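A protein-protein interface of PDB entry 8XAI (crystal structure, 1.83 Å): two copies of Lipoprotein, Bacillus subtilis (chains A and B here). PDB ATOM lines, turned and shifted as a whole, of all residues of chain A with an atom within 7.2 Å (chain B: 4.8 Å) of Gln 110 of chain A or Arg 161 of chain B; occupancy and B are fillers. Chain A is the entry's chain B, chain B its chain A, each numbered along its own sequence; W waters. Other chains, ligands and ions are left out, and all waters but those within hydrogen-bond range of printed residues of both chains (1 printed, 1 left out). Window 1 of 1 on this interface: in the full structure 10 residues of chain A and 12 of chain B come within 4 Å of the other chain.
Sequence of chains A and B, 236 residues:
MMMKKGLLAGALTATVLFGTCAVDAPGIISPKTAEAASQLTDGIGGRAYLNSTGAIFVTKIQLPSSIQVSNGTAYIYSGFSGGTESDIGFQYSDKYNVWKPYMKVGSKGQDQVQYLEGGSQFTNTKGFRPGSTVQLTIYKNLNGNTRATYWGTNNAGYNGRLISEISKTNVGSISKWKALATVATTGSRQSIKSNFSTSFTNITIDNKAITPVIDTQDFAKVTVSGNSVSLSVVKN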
ATOM      1  N   ASP A  87     -12.411  21.149  35.791  1.00  0.00           N
ATOM      2  CA  ASP A  87     -10.949  21.108  35.808  1.00  0.00           C
ATOM      3  C   ASP A  87     -10.472  21.231  34.366  1.00  0.00           C
ATOM      4  O   ASP A  87     -10.671  20.306  33.565  1.00  0.00           O
ATOM      5  CB  ASP A  87     -10.421  19.815  36.435  1.00  0.00           C
ATOM      6  CG  ASP A  87     -10.738  19.687  37.892  1.00  0.00           C
ATOM      7  OD1 ASP A  87     -11.152  20.689  38.512  1.00  0.00           O
ATOM      8  OD2 ASP A  87     -10.506  18.578  38.430  1.00  0.00           O
ATOM      9  N   GLY A  89      -7.234  22.409  31.841  1.00  0.00           N
ATOM     10  CA  GLY A  89      -5.860  22.824  31.641  1.00  0.00           C
ATOM     11  C   GLY A  89      -5.017  21.712  31.052  1.00  0.00           C
ATOM     12  O   GLY A  89      -5.270  21.252  29.940  1.00  0.00           O
ATOM     13  N   GLN A  91      -2.335  18.090  31.753  1.00  0.00           N
ATOM     14  CA  GLN A  91      -1.814  17.067  32.642  1.00  0.00           C
ATOM     15  C   GLN A  91      -0.470  16.576  32.093  1.00  0.00           C
ATOM     16  O   GLN A  91      -0.277  16.483  30.868  1.00  0.00           O
ATOM     17  CB  GLN A  91      -2.814  15.914  32.794  1.00  0.00           C
ATOM     18  CG  GLN A  91      -2.442  14.681  32.068  1.00  0.00           C
ATOM     19  CD  GLN A  91      -3.480  13.569  32.164  1.00  0.00           C
ATOM     20  OE1 GLN A  91      -4.240  13.346  31.224  1.00  0.00           O
ATOM     21  NE2 GLN A  91      -3.561  12.922  33.316  1.00  0.00           N
ATOM     22  N   LYS A 100      -0.192  17.490  28.244  1.00  0.00           N
ATOM     23  CA  LYS A 100      -1.311  17.151  27.406  1.00  0.00           C
ATOM     24  C   LYS A 100      -2.516  17.987  27.807  1.00  0.00           C
ATOM     25  O   LYS A 100      -2.674  18.329  28.983  1.00  0.00           O
ATOM     26  CB  LYS A 100      -1.675  15.677  27.546  1.00  0.00           C
ATOM     27  CG  LYS A 100      -0.600  14.703  27.139  1.00  0.00           C
ATOM     28  CD  LYS A 100      -1.004  13.329  27.624  1.00  0.00           C
ATOM     29  CE  LYS A 100      -1.603  13.353  29.017  1.00  0.00           C
ATOM     30  NZ  LYS A 100      -0.666  13.029  30.141  1.00  0.00           N
ATOM     31  N   PRO A 101      -3.381  18.311  26.855  1.00  0.00           N
ATOM     32  CA  PRO A 101      -4.590  19.055  27.193  1.00  0.00           C
ATOM     33  C   PRO A 101      -5.463  18.185  28.073  1.00  0.00           C
ATOM     34  O   PRO A 101      -5.479  16.958  27.944  1.00  0.00           O
ATOM     35  CB  PRO A 101      -5.242  19.300  25.829  1.00  0.00           C
ATOM     36  CG  PRO A 101      -4.611  18.283  24.933  1.00  0.00           C
ATOM     37  CD  PRO A 101      -3.211  18.217  25.397  1.00  0.00           C
ATOM     38  N   TYR A 102      -6.171  18.831  28.999  1.00  0.00           N
ATOM     39  CA  TYR A 102      -6.980  18.086  29.951  1.00  0.00           C
ATOM     40  C   TYR A 102      -8.212  18.887  30.299  1.00  0.00           C
ATOM     41  O   TYR A 102      -8.107  20.075  30.621  1.00  0.00           O
ATOM     42  CB  TYR A 102      -6.222  17.787  31.236  1.00  0.00           C
ATOM     43  CG  TYR A 102      -7.087  17.067  32.237  1.00  0.00           C
ATOM     44  CD1 TYR A 102      -7.277  15.694  32.135  1.00  0.00           C
ATOM     45  CD2 TYR A 102      -7.754  17.746  33.254  1.00  0.00           C
ATOM     46  CE1 TYR A 102      -8.060  15.013  33.035  1.00  0.00           C
ATOM     47  CE2 TYR A 102      -8.569  17.053  34.152  1.00  0.00           C
ATOM     48  CZ  TYR A 102      -8.703  15.692  34.034  1.00  0.00           C
ATOM     49  OH  TYR A 102      -9.481  14.984  34.920  1.00  0.00           O
ATOM     50  N   MET A 103      -9.372  18.239  30.259  1.00  0.00           N
ATOM     51  CA  MET A 103     -10.593  18.929  30.629  1.00  0.00           C
ATOM     52  C   MET A 103     -11.593  17.913  31.158  1.00  0.00           C
ATOM     53  O   MET A 103     -11.759  16.823  30.599  1.00  0.00           O
ATOM     54  CB  MET A 103     -11.172  19.735  29.454  1.00  0.00           C
ATOM     55  CG  MET A 103     -12.605  20.235  29.690  1.00  0.00           C
ATOM     56  SD  MET A 103     -13.252  21.466  28.516  1.00  0.00           S
ATOM     57  CE  MET A 103     -12.640  20.803  26.970  1.00  0.00           C
ATOM     58  N   LYS A 104     -12.220  18.281  32.269  1.00  0.00           N
ATOM     59  CA  LYS A 104     -13.308  17.528  32.882  1.00  0.00           C
ATOM     60  C   LYS A 104     -14.326  18.540  33.390  1.00  0.00           C
ATOM     61  O   LYS A 104     -13.977  19.461  34.140  1.00  0.00           O
ATOM     62  CB  LYS A 104     -12.768  16.636  34.013  1.00  0.00           C
ATOM     63  CG  LYS A 104     -13.746  16.180  35.102  1.00  0.00           C
ATOM     64  CD  LYS A 104     -14.724  15.141  34.593  1.00  0.00           C
ATOM     65  CE  LYS A 104     -15.246  14.220  35.712  1.00  0.00           C
ATOM     66  NZ  LYS A 104     -14.240  13.867  36.760  1.00  0.00           N
ATOM     67  N   VAL A 105     -15.583  18.395  32.969  1.00  0.00           N
ATOM     68  CA  VAL A 105     -16.641  19.313  33.382  1.00  0.00           C
ATOM     69  C   VAL A 105     -17.753  18.479  33.984  1.00  0.00           C
ATOM     70  O   VAL A 105     -18.347  17.643  33.293  1.00  0.00           O
ATOM     71  CB  VAL A 105     -17.180  20.166  32.225  1.00  0.00           C
ATOM     72  CG1 VAL A 105     -18.359  20.987  32.713  1.00  0.00           C
ATOM     73  CG2 VAL A 105     -16.102  21.097  31.681  1.00  0.00           C
ATOM     74  N   SER A 107     -19.480  15.587  35.474  1.00  0.00           N
ATOM     75  CA  SER A 107     -19.154  14.175  35.534  1.00  0.00           C
ATOM     76  C   SER A 107     -18.544  13.650  34.247  1.00  0.00           C
ATOM     77  O   SER A 107     -17.964  12.558  34.252  1.00  0.00           O
ATOM     78  CB  SER A 107     -20.404  13.364  35.896  1.00  0.00           C
ATOM     79  OG  SER A 107     -21.482  13.642  35.028  1.00  0.00           O
ATOM     80  N   LYS A 108     -18.644  14.381  33.152  1.00  0.00           N
ATOM     81  CA  LYS A 108     -18.136  13.893  31.879  1.00  0.00           C
ATOM     82  C   LYS A 108     -16.748  14.470  31.629  1.00  0.00           C
ATOM     83  O   LYS A 108     -16.536  15.681  31.756  1.00  0.00           O
ATOM     84  CB  LYS A 108     -19.165  14.158  30.776  1.00  0.00           C
ATOM     85  CG  LYS A 108     -20.029  15.411  30.927  1.00  0.00           C
ATOM     86  CD  LYS A 108     -20.489  15.988  29.602  1.00  0.00           C
ATOM     87  CE  LYS A 108     -21.896  15.420  29.287  1.00  0.00           C
ATOM     88  NZ  LYS A 108     -22.715  16.225  28.337  1.00  0.00           N
ATOM     89  N   GLY A 109     -15.786  13.578  31.381  1.00  0.00           N
ATOM     90  CA  GLY A 109     -14.373  13.909  31.402  1.00  0.00           C
ATOM     91  C   GLY A 109     -13.619  13.665  30.104  1.00  0.00           C
ATOM     92  O   GLY A 109     -14.202  13.745  29.021  1.00  0.00           O
ATOM     93  N   GLN A 110     -12.318  13.370  30.214  1.00  0.00           N
ATOM     94  CA  GLN A 110     -11.443  13.227  29.043  1.00  0.00           C
ATOM     95  C   GLN A 110     -12.010  12.330  27.944  1.00  0.00           C
ATOM     96  O   GLN A 110     -11.791  12.596  26.759  1.00  0.00           O
ATOM     97  CB  GLN A 110     -10.076  12.708  29.479  1.00  0.00           C
ATOM     98  CG  GLN A 110      -9.124  13.801  29.978  1.00  0.00           C
ATOM     99  CD  GLN A 110      -8.674  14.703  28.833  1.00  0.00           C
ATOM    100  OE1 GLN A 110      -9.199  15.773  28.618  1.00  0.00           O
ATOM    101  NE2 GLN A 110      -7.675  14.244  28.087  1.00  0.00           N
ATOM    102  N   ASP A 111     -12.727  11.268  28.300  1.00  0.00           N
ATOM    103  CA  ASP A 111     -13.263  10.431  27.239  1.00  0.00           C
ATOM    104  C   ASP A 111     -14.338  11.125  26.418  1.00  0.00           C
ATOM    105  O   ASP A 111     -14.621  10.673  25.305  1.00  0.00           O
ATOM    106  CB  ASP A 111     -13.816   9.106  27.784  1.00  0.00           C
ATOM    107  CG  ASP A 111     -14.019   8.099  26.678  1.00  0.00           C
ATOM    108  OD1 ASP A 111     -13.136   7.993  25.806  1.00  0.00           O
ATOM    109  OD2 ASP A 111     -15.072   7.434  26.650  1.00  0.00           O
ATOM    110  N   GLN A 112     -14.910  12.222  26.903  1.00  0.00           N
ATOM    111  CA  GLN A 112     -15.911  12.965  26.143  1.00  0.00           C
ATOM    112  C   GLN A 112     -15.438  14.356  25.725  1.00  0.00           C
ATOM    113  O   GLN A 112     -16.270  15.219  25.394  1.00  0.00           O
ATOM    114  CB  GLN A 112     -17.207  13.041  26.943  1.00  0.00           C
ATOM    115  CG  GLN A 112     -17.655  11.639  27.384  1.00  0.00           C
ATOM    116  CD  GLN A 112     -18.990  11.662  28.058  1.00  0.00           C
ATOM    117  OE1 GLN A 112     -19.050  11.511  29.263  1.00  0.00           O
ATOM    118  NE2 GLN A 112     -20.064  11.788  27.292  1.00  0.00           N
ATOM    119  N   VAL A 113     -14.122  14.585  25.715  1.00  0.00           N
ATOM    120  CA  VAL A 113     -13.547  15.763  25.060  1.00  0.00           C
ATOM    121  C   VAL A 113     -13.390  15.526  23.561  1.00  0.00           C
ATOM    122  O   VAL A 113     -12.748  14.563  23.129  1.00  0.00           O
ATOM    123  CB  VAL A 113     -12.218  16.180  25.712  1.00  0.00           C
ATOM    124  CG1 VAL A 113     -11.106  15.233  25.336  1.00  0.00           C
ATOM    125  CG2 VAL A 113     -11.790  17.520  25.105  1.00  0.00           C
ATOM    126  N   GLN A 114     -13.984  16.405  22.755  1.00  0.00           N
ATOM    127  CA  GLN A 114     -13.691  16.424  21.328  1.00  0.00           C
ATOM    128  C   GLN A 114     -12.787  17.596  20.968  1.00  0.00           C
ATOM    129  O   GLN A 114     -12.774  18.634  21.629  1.00  0.00           O
ATOM    130  CB  GLN A 114     -14.957  16.455  20.463  1.00  0.00           C
ATOM    131  CG  GLN A 114     -15.951  17.559  20.741  1.00  0.00           C
ATOM    132  CD  GLN A 114     -17.137  17.511  19.772  1.00  0.00           C
ATOM    133  OE1 GLN A 114     -17.565  16.432  19.364  1.00  0.00           O
ATOM    134  NE2 GLN A 114     -17.694  18.682  19.439  1.00  0.00           N
ATOM    135  N   TYR A 115     -12.018  17.418  19.902  1.00  0.00           N
ATOM    136  CA  TYR A 115     -11.015  18.395  19.513  1.00  0.00           C
ATOM    137  C   TYR A 115     -11.423  18.932  18.153  1.00  0.00           C
ATOM    138  O   TYR A 115     -11.337  18.221  17.151  1.00  0.00           O
ATOM    139  CB  TYR A 115      -9.614  17.775  19.523  1.00  0.00           C
ATOM    140  CG  TYR A 115      -9.238  17.238  20.896  1.00  0.00           C
ATOM    141  CD1 TYR A 115      -8.933  18.111  21.933  1.00  0.00           C
ATOM    142  CD2 TYR A 115      -9.199  15.873  21.158  1.00  0.00           C
ATOM    143  CE1 TYR A 115      -8.595  17.645  23.189  1.00  0.00           C
ATOM    144  CE2 TYR A 115      -8.860  15.403  22.398  1.00  0.00           C
ATOM    145  CZ  TYR A 115      -8.561  16.297  23.418  1.00  0.00           C
ATOM    146  OH  TYR A 115      -8.203  15.834  24.663  1.00  0.00           O
ATOM    147  N   THR A 123      -2.543  16.343  20.503  1.00  0.00           N
ATOM    148  CA  THR A 123      -3.113  15.215  21.223  1.00  0.00           C
ATOM    149  C   THR A 123      -2.492  13.912  20.723  1.00  0.00           C
ATOM    150  O   THR A 123      -1.683  13.889  19.786  1.00  0.00           O
ATOM    151  CB  THR A 123      -4.650  15.174  21.107  1.00  0.00           C
ATOM    152  OG1 THR A 123      -5.030  14.681  19.813  1.00  0.00           O
ATOM    153  CG2 THR A 123      -5.283  16.530  21.365  1.00  0.00           C
ATOM    154  N   ASN A 124      -2.896  12.824  21.385  1.00  0.00           N
ATOM    155  CA  ASN A 124      -2.309  11.486  21.356  1.00  0.00           C
ATOM    156  C   ASN A 124      -0.965  11.062  21.902  1.00  0.00           C
ATOM    157  O   ASN A 124      -0.865  10.115  22.695  1.00  0.00           O
ATOM    158  CB  ASN A 124      -2.130  10.979  19.935  1.00  0.00           C
ATOM    159  CG  ASN A 124      -3.436  10.668  19.303  1.00  0.00           C
ATOM    160  OD1 ASN A 124      -3.785   9.495  19.160  1.00  0.00           O
ATOM    161  ND2 ASN A 124      -4.185  11.697  18.928  1.00  0.00           N
ATOM    162  N   TYR A 150      -6.427  26.589  23.253  1.00  0.00           N
ATOM    163  CA  TYR A 150      -5.008  26.686  23.581  1.00  0.00           C
ATOM    164  C   TYR A 150      -4.253  27.256  22.385  1.00  0.00           C
ATOM    165  O   TYR A 150      -4.426  26.785  21.252  1.00  0.00           O
ATOM    166  CB  TYR A 150      -4.430  25.308  23.929  1.00  0.00           C
ATOM    167  CG  TYR A 150      -5.144  24.508  25.022  1.00  0.00           C
ATOM    168  CD1 TYR A 150      -6.405  23.965  24.802  1.00  0.00           C
ATOM    169  CD2 TYR A 150      -4.500  24.199  26.225  1.00  0.00           C
ATOM    170  CE1 TYR A 150      -7.041  23.213  25.768  1.00  0.00           C
ATOM    171  CE2 TYR A 150      -5.135  23.445  27.213  1.00  0.00           C
ATOM    172  CZ  TYR A 150      -6.405  22.943  26.965  1.00  0.00           C
ATOM    173  OH  TYR A 150      -7.057  22.167  27.877  1.00  0.00           O
ATOM    174  N   SER A 164     -10.656  22.586  22.076  1.00  0.00           N
ATOM    175  CA  SER A 164     -11.261  21.409  22.680  1.00  0.00           C
ATOM    176  C   SER A 164     -12.603  21.783  23.272  1.00  0.00           C
ATOM    177  O   SER A 164     -12.842  22.929  23.636  1.00  0.00           O
ATOM    178  CB  SER A 164     -10.413  20.811  23.797  1.00  0.00           C
ATOM    179  OG  SER A 164     -10.140  21.764  24.800  1.00  0.00           O
ATOM    180  N   ILE A 166     -16.195  20.126  25.569  1.00  0.00           N
ATOM    181  CA  ILE A 166     -17.202  19.139  25.959  1.00  0.00           C
ATOM    182  C   ILE A 166     -18.569  19.698  25.606  1.00  0.00           C
ATOM    183  O   ILE A 166     -18.873  20.852  25.922  1.00  0.00           O
ATOM    184  CB  ILE A 166     -17.134  18.769  27.441  1.00  0.00           C
ATOM    185  CG1 ILE A 166     -15.880  17.953  27.682  1.00  0.00           C
ATOM    186  CG2 ILE A 166     -18.321  17.872  27.795  1.00  0.00           C
ATOM    187  CD1 ILE A 166     -15.209  18.329  28.905  1.00  0.00           C
ATOM    188  N   GLU B 117      -8.569   3.585  25.906  1.00  0.00           N
ATOM    189  CA  GLU B 117      -9.593   4.481  26.422  1.00  0.00           C
ATOM    190  C   GLU B 117     -10.933   4.100  25.811  1.00  0.00           C
ATOM    191  O   GLU B 117     -10.998   3.788  24.616  1.00  0.00           O
ATOM    192  CB  GLU B 117      -9.316   5.953  26.080  1.00  0.00           C
ATOM    193  CG  GLU B 117     -10.026   6.930  27.004  1.00  0.00           C
ATOM    194  CD  GLU B 117      -9.840   8.370  26.579  1.00  0.00           C
ATOM    195  OE1 GLU B 117      -9.435   8.611  25.418  1.00  0.00           O
ATOM    196  OE2 GLU B 117     -10.049   9.270  27.421  1.00  0.00           O
ATOM    197  N   GLY B 118     -11.997   4.177  26.620  1.00  0.00           N
ATOM    198  CA  GLY B 118     -13.362   3.945  26.165  1.00  0.00           C
ATOM    199  C   GLY B 118     -13.775   2.493  26.084  1.00  0.00           C
ATOM    200  O   GLY B 118     -14.899   2.203  25.638  1.00  0.00           O
ATOM    201  N   PHE B 122     -17.580   0.792  24.521  1.00  0.00           N
ATOM    202  CA  PHE B 122     -17.670   0.421  23.109  1.00  0.00           C
ATOM    203  C   PHE B 122     -17.162  -0.965  22.758  1.00  0.00           C
ATOM    204  O   PHE B 122     -17.062  -1.284  21.570  1.00  0.00           O
ATOM    205  CB  PHE B 122     -16.921   1.425  22.216  1.00  0.00           C
ATOM    206  CG  PHE B 122     -17.366   2.827  22.374  1.00  0.00           C
ATOM    207  CD1 PHE B 122     -18.521   3.253  21.745  1.00  0.00           C
ATOM    208  CD2 PHE B 122     -16.619   3.737  23.106  1.00  0.00           C
ATOM    209  CE1 PHE B 122     -18.960   4.607  21.865  1.00  0.00           C
ATOM    210  CE2 PHE B 122     -17.026   5.067  23.215  1.00  0.00           C
ATOM    211  CZ  PHE B 122     -18.219   5.495  22.587  1.00  0.00           C
ATOM    212  N   THR B 149      -8.666   5.509  16.346  1.00  0.00           N
ATOM    213  CA  THR B 149      -9.443   6.264  17.315  1.00  0.00           C
ATOM    214  C   THR B 149     -10.836   6.502  16.769  1.00  0.00           C
ATOM    215  O   THR B 149     -10.989   6.951  15.628  1.00  0.00           O
ATOM    216  CB  THR B 149      -8.763   7.583  17.643  1.00  0.00           C
ATOM    217  OG1 THR B 149      -7.486   7.311  18.252  1.00  0.00           O
ATOM    218  CG2 THR B 149      -9.631   8.459  18.503  1.00  0.00           C
ATOM    219  N   TYR B 150     -11.841   6.177  17.579  1.00  0.00           N
ATOM    220  CA  TYR B 150     -13.227   6.341  17.186  1.00  0.00           C
ATOM    221  C   TYR B 150     -13.882   7.400  18.074  1.00  0.00           C
ATOM    222  O   TYR B 150     -13.725   7.394  19.304  1.00  0.00           O
ATOM    223  CB  TYR B 150     -14.019   5.025  17.299  1.00  0.00           C
ATOM    224  CG  TYR B 150     -13.456   3.775  16.613  1.00  0.00           C
ATOM    225  CD1 TYR B 150     -12.268   3.176  17.062  1.00  0.00           C
ATOM    226  CD2 TYR B 150     -14.123   3.180  15.546  1.00  0.00           C
ATOM    227  CE1 TYR B 150     -11.754   2.029  16.460  1.00  0.00           C
ATOM    228  CE2 TYR B 150     -13.618   2.012  14.929  1.00  0.00           C
ATOM    229  CZ  TYR B 150     -12.423   1.449  15.394  1.00  0.00           C
ATOM    230  OH  TYR B 150     -11.884   0.310  14.821  1.00  0.00           O
ATOM    231  N   TRP B 151     -14.628   8.299  17.458  1.00  0.00           N
ATOM    232  CA  TRP B 151     -15.520   9.179  18.197  1.00  0.00           C
ATOM    233  C   TRP B 151     -16.928   8.806  17.763  1.00  0.00           C
ATOM    234  O   TRP B 151     -17.201   8.759  16.559  1.00  0.00           O
ATOM    235  CB  TRP B 151     -15.208  10.659  17.926  1.00  0.00           C
ATOM    236  CG  TRP B 151     -16.158  11.528  18.624  1.00  0.00           C
ATOM    237  CD1 TRP B 151     -17.339  12.019  18.130  1.00  0.00           C
ATOM    238  CD2 TRP B 151     -16.074  11.943  19.981  1.00  0.00           C
ATOM    239  NE1 TRP B 151     -17.980  12.742  19.105  1.00  0.00           N
ATOM    240  CE2 TRP B 151     -17.227  12.707  20.254  1.00  0.00           C
ATOM    241  CE3 TRP B 151     -15.123  11.751  21.004  1.00  0.00           C
ATOM    242  CZ2 TRP B 151     -17.461  13.297  21.510  1.00  0.00           C
ATOM    243  CZ3 TRP B 151     -15.360  12.325  22.256  1.00  0.00           C
ATOM    244  CH2 TRP B 151     -16.519  13.098  22.490  1.00  0.00           C
ATOM    245  N   GLY B 160     -18.635   9.291  23.127  1.00  0.00           N
ATOM    246  CA  GLY B 160     -17.258   9.300  23.608  1.00  0.00           C
ATOM    247  C   GLY B 160     -16.224   8.743  22.628  1.00  0.00           C
ATOM    248  O   GLY B 160     -16.502   8.503  21.454  1.00  0.00           O
ATOM    249  N   ARG B 161     -15.016   8.543  23.156  1.00  0.00           N
ATOM    250  CA  ARG B 161     -13.837   8.113  22.415  1.00  0.00           C
ATOM    251  C   ARG B 161     -13.482   6.677  22.782  1.00  0.00           C
ATOM    252  O   ARG B 161     -13.500   6.292  23.951  1.00  0.00           O
ATOM    253  CB  ARG B 161     -12.625   9.005  22.728  1.00  0.00           C
ATOM    254  CG  ARG B 161     -11.338   8.721  21.922  1.00  0.00           C
ATOM    255  CD  ARG B 161     -10.416   9.938  22.037  1.00  0.00           C
ATOM    256  NE  ARG B 161     -10.916  11.031  21.220  1.00  0.00           N
ATOM    257  CZ  ARG B 161     -11.416  12.151  21.715  1.00  0.00           C
ATOM    258  NH1 ARG B 161     -11.518  12.341  23.025  1.00  0.00           N
ATOM    259  NH2 ARG B 161     -11.872  13.081  20.880  1.00  0.00           N
ATOM    260  N   LEU B 162     -13.175   5.883  21.775  1.00  0.00           N
ATOM    261  CA  LEU B 162     -12.446   4.648  21.974  1.00  0.00           C
ATOM    262  C   LEU B 162     -11.076   4.811  21.324  1.00  0.00           C
ATOM    263  O   LEU B 162     -10.980   5.278  20.183  1.00  0.00           O
ATOM    264  CB  LEU B 162     -13.217   3.476  21.392  1.00  0.00           C
ATOM    265  CG  LEU B 162     -12.599   2.081  21.437  1.00  0.00           C
ATOM    266  CD1 LEU B 162     -12.532   1.515  22.854  1.00  0.00           C
ATOM    267  CD2 LEU B 162     -13.439   1.202  20.601  1.00  0.00           C
ATOM    268  N   ILE B 163     -10.015   4.478  22.066  1.00  0.00           N
ATOM    269  CA  ILE B 163      -8.666   4.392  21.512  1.00  0.00           C
ATOM    270  C   ILE B 163      -8.293   2.924  21.492  1.00  0.00           C
ATOM    271  O   ILE B 163      -8.236   2.287  22.546  1.00  0.00           O
ATOM    272  CB  ILE B 163      -7.625   5.174  22.332  1.00  0.00           C
ATOM    273  CG1 ILE B 163      -7.991   6.654  22.461  1.00  0.00           C
ATOM    274  CG2 ILE B 163      -6.261   5.064  21.677  1.00  0.00           C
ATOM    275  CD1 ILE B 163      -7.724   7.392  21.301  1.00  0.00           C
HETATM  276  O   HOH W   1     -12.199  15.176  18.727  1.00  0.00           O
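The side-chain carboxylate of Glu 117 of chain B sits close to the backbone NH of Asp 111 of chain A (3.5 Å). N of Arg 161 of chain B lies within hydrogen-bond range of O of Asp 111 of chain A (3.1 Å). The guanidinium group (NH1) of Arg 161 of chain B is in hydrogen-bond range of the backbone carbonyl oxygen (O) of Val 113 of chain A, at 2.5 Å.
O of Glu 117 of chain B is in hydrogen-bond range of N of Ile 163 of chain B. O of Pro 101 of chain A sits at hydrogen-bond distance from NE2 of Gln 110 of chain A (3.5 Å). The backbone NH of Met 103 of chain A lies within hydrogen-bond range of the side-chain amide oxygen of Gln 110 of chain A (3.0 Å).
Of the 23 printed residues of chain A, 6 touch a printed residue of chain B. Printed residues of chain A that touch a printed residue of chain B: Gln 110, Asp 111, Gln 112, Val 113, Gln 114 and Tyr 115. Hydrophobic or aromatic side chains of chain A that line the printed part of chain B: Val 113 and Tyr 115. Among the printed residues, no Asp or Glu carboxylate lies within 4 Å of a Lys or Arg side-chain nitrogen of the other chain.
Of chain B, only Glu 117 (3.7 Å) and Arg 161 (3.8 Å) come within 4 Å of Gln 110 of chain A. Of chain A, only Gln 110, Asp 111, Val 113, Gln 114 and Tyr 115 come within 4 Å of Arg 161 of chain B. Of the printed residues of chain B, Val 113 of chain A touches Trp 151 (3.5 Å) and Arg 161 (2.5 Å). Of the printed residues of chain A, Gly 160 of chain B touches Asp 111 (3.4 Å). Of the printed residues of chain B, Gln 112 of chain A touches Trp 151 (3.6 Å). Of the printed residues of chain B, Asp 111 of chain A touches Glu 117 (3.4 Å), Gly 118 (3.9 Å), Trp 151 (3.5 Å), Gly 160 (3.4 Å) and Arg 161 (2.5 Å). Ile 163 of chain B touches none of the printed residues of chain A. Tyr 150 of chain A touches none of the printed residues of chain B. The nearest printed residue of chain B that does not touch Val 113 of chain A is Glu 117 of chain B (6.4 Å).
1 position is printed for both chains. Of the 13 pairs that touch across the chains among the printed residues, none has its exchanged pair printed and touching as well.
Water W1 bridges the backbone NH of Tyr 115 of chain A (2.5 Å) and the guanidinium group of Arg 161 of chain B (3.0 Å).
Among the printed residues, pairs that only touch across the chains: Asp 111 of chain A with Gly 160 of chain B (3.4 Å), Asp 111 of chain A with Trp 151 of chain B (3.5 Å), Val 113 of chain A with Trp 151 of chain B (3.5 Å), Gln 112 of chain A with Trp 151 of chain B (3.6 Å), Gln 110 of chain A with Glu 117 of chain B (3.7 Å), Gln 114 of chain A with Trp 151 of chain B (3.7 Å), Gln 110 of chain A with Arg 161 of chain B (3.8 Å), Gln 114 of chain A with Arg 161 of chain B (3.8 Å), Tyr 115 of chain A with Arg 161 of chain B (3.9 Å) and Asp 111 of chain A with Gly 118 of chain B (3.9 Å).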
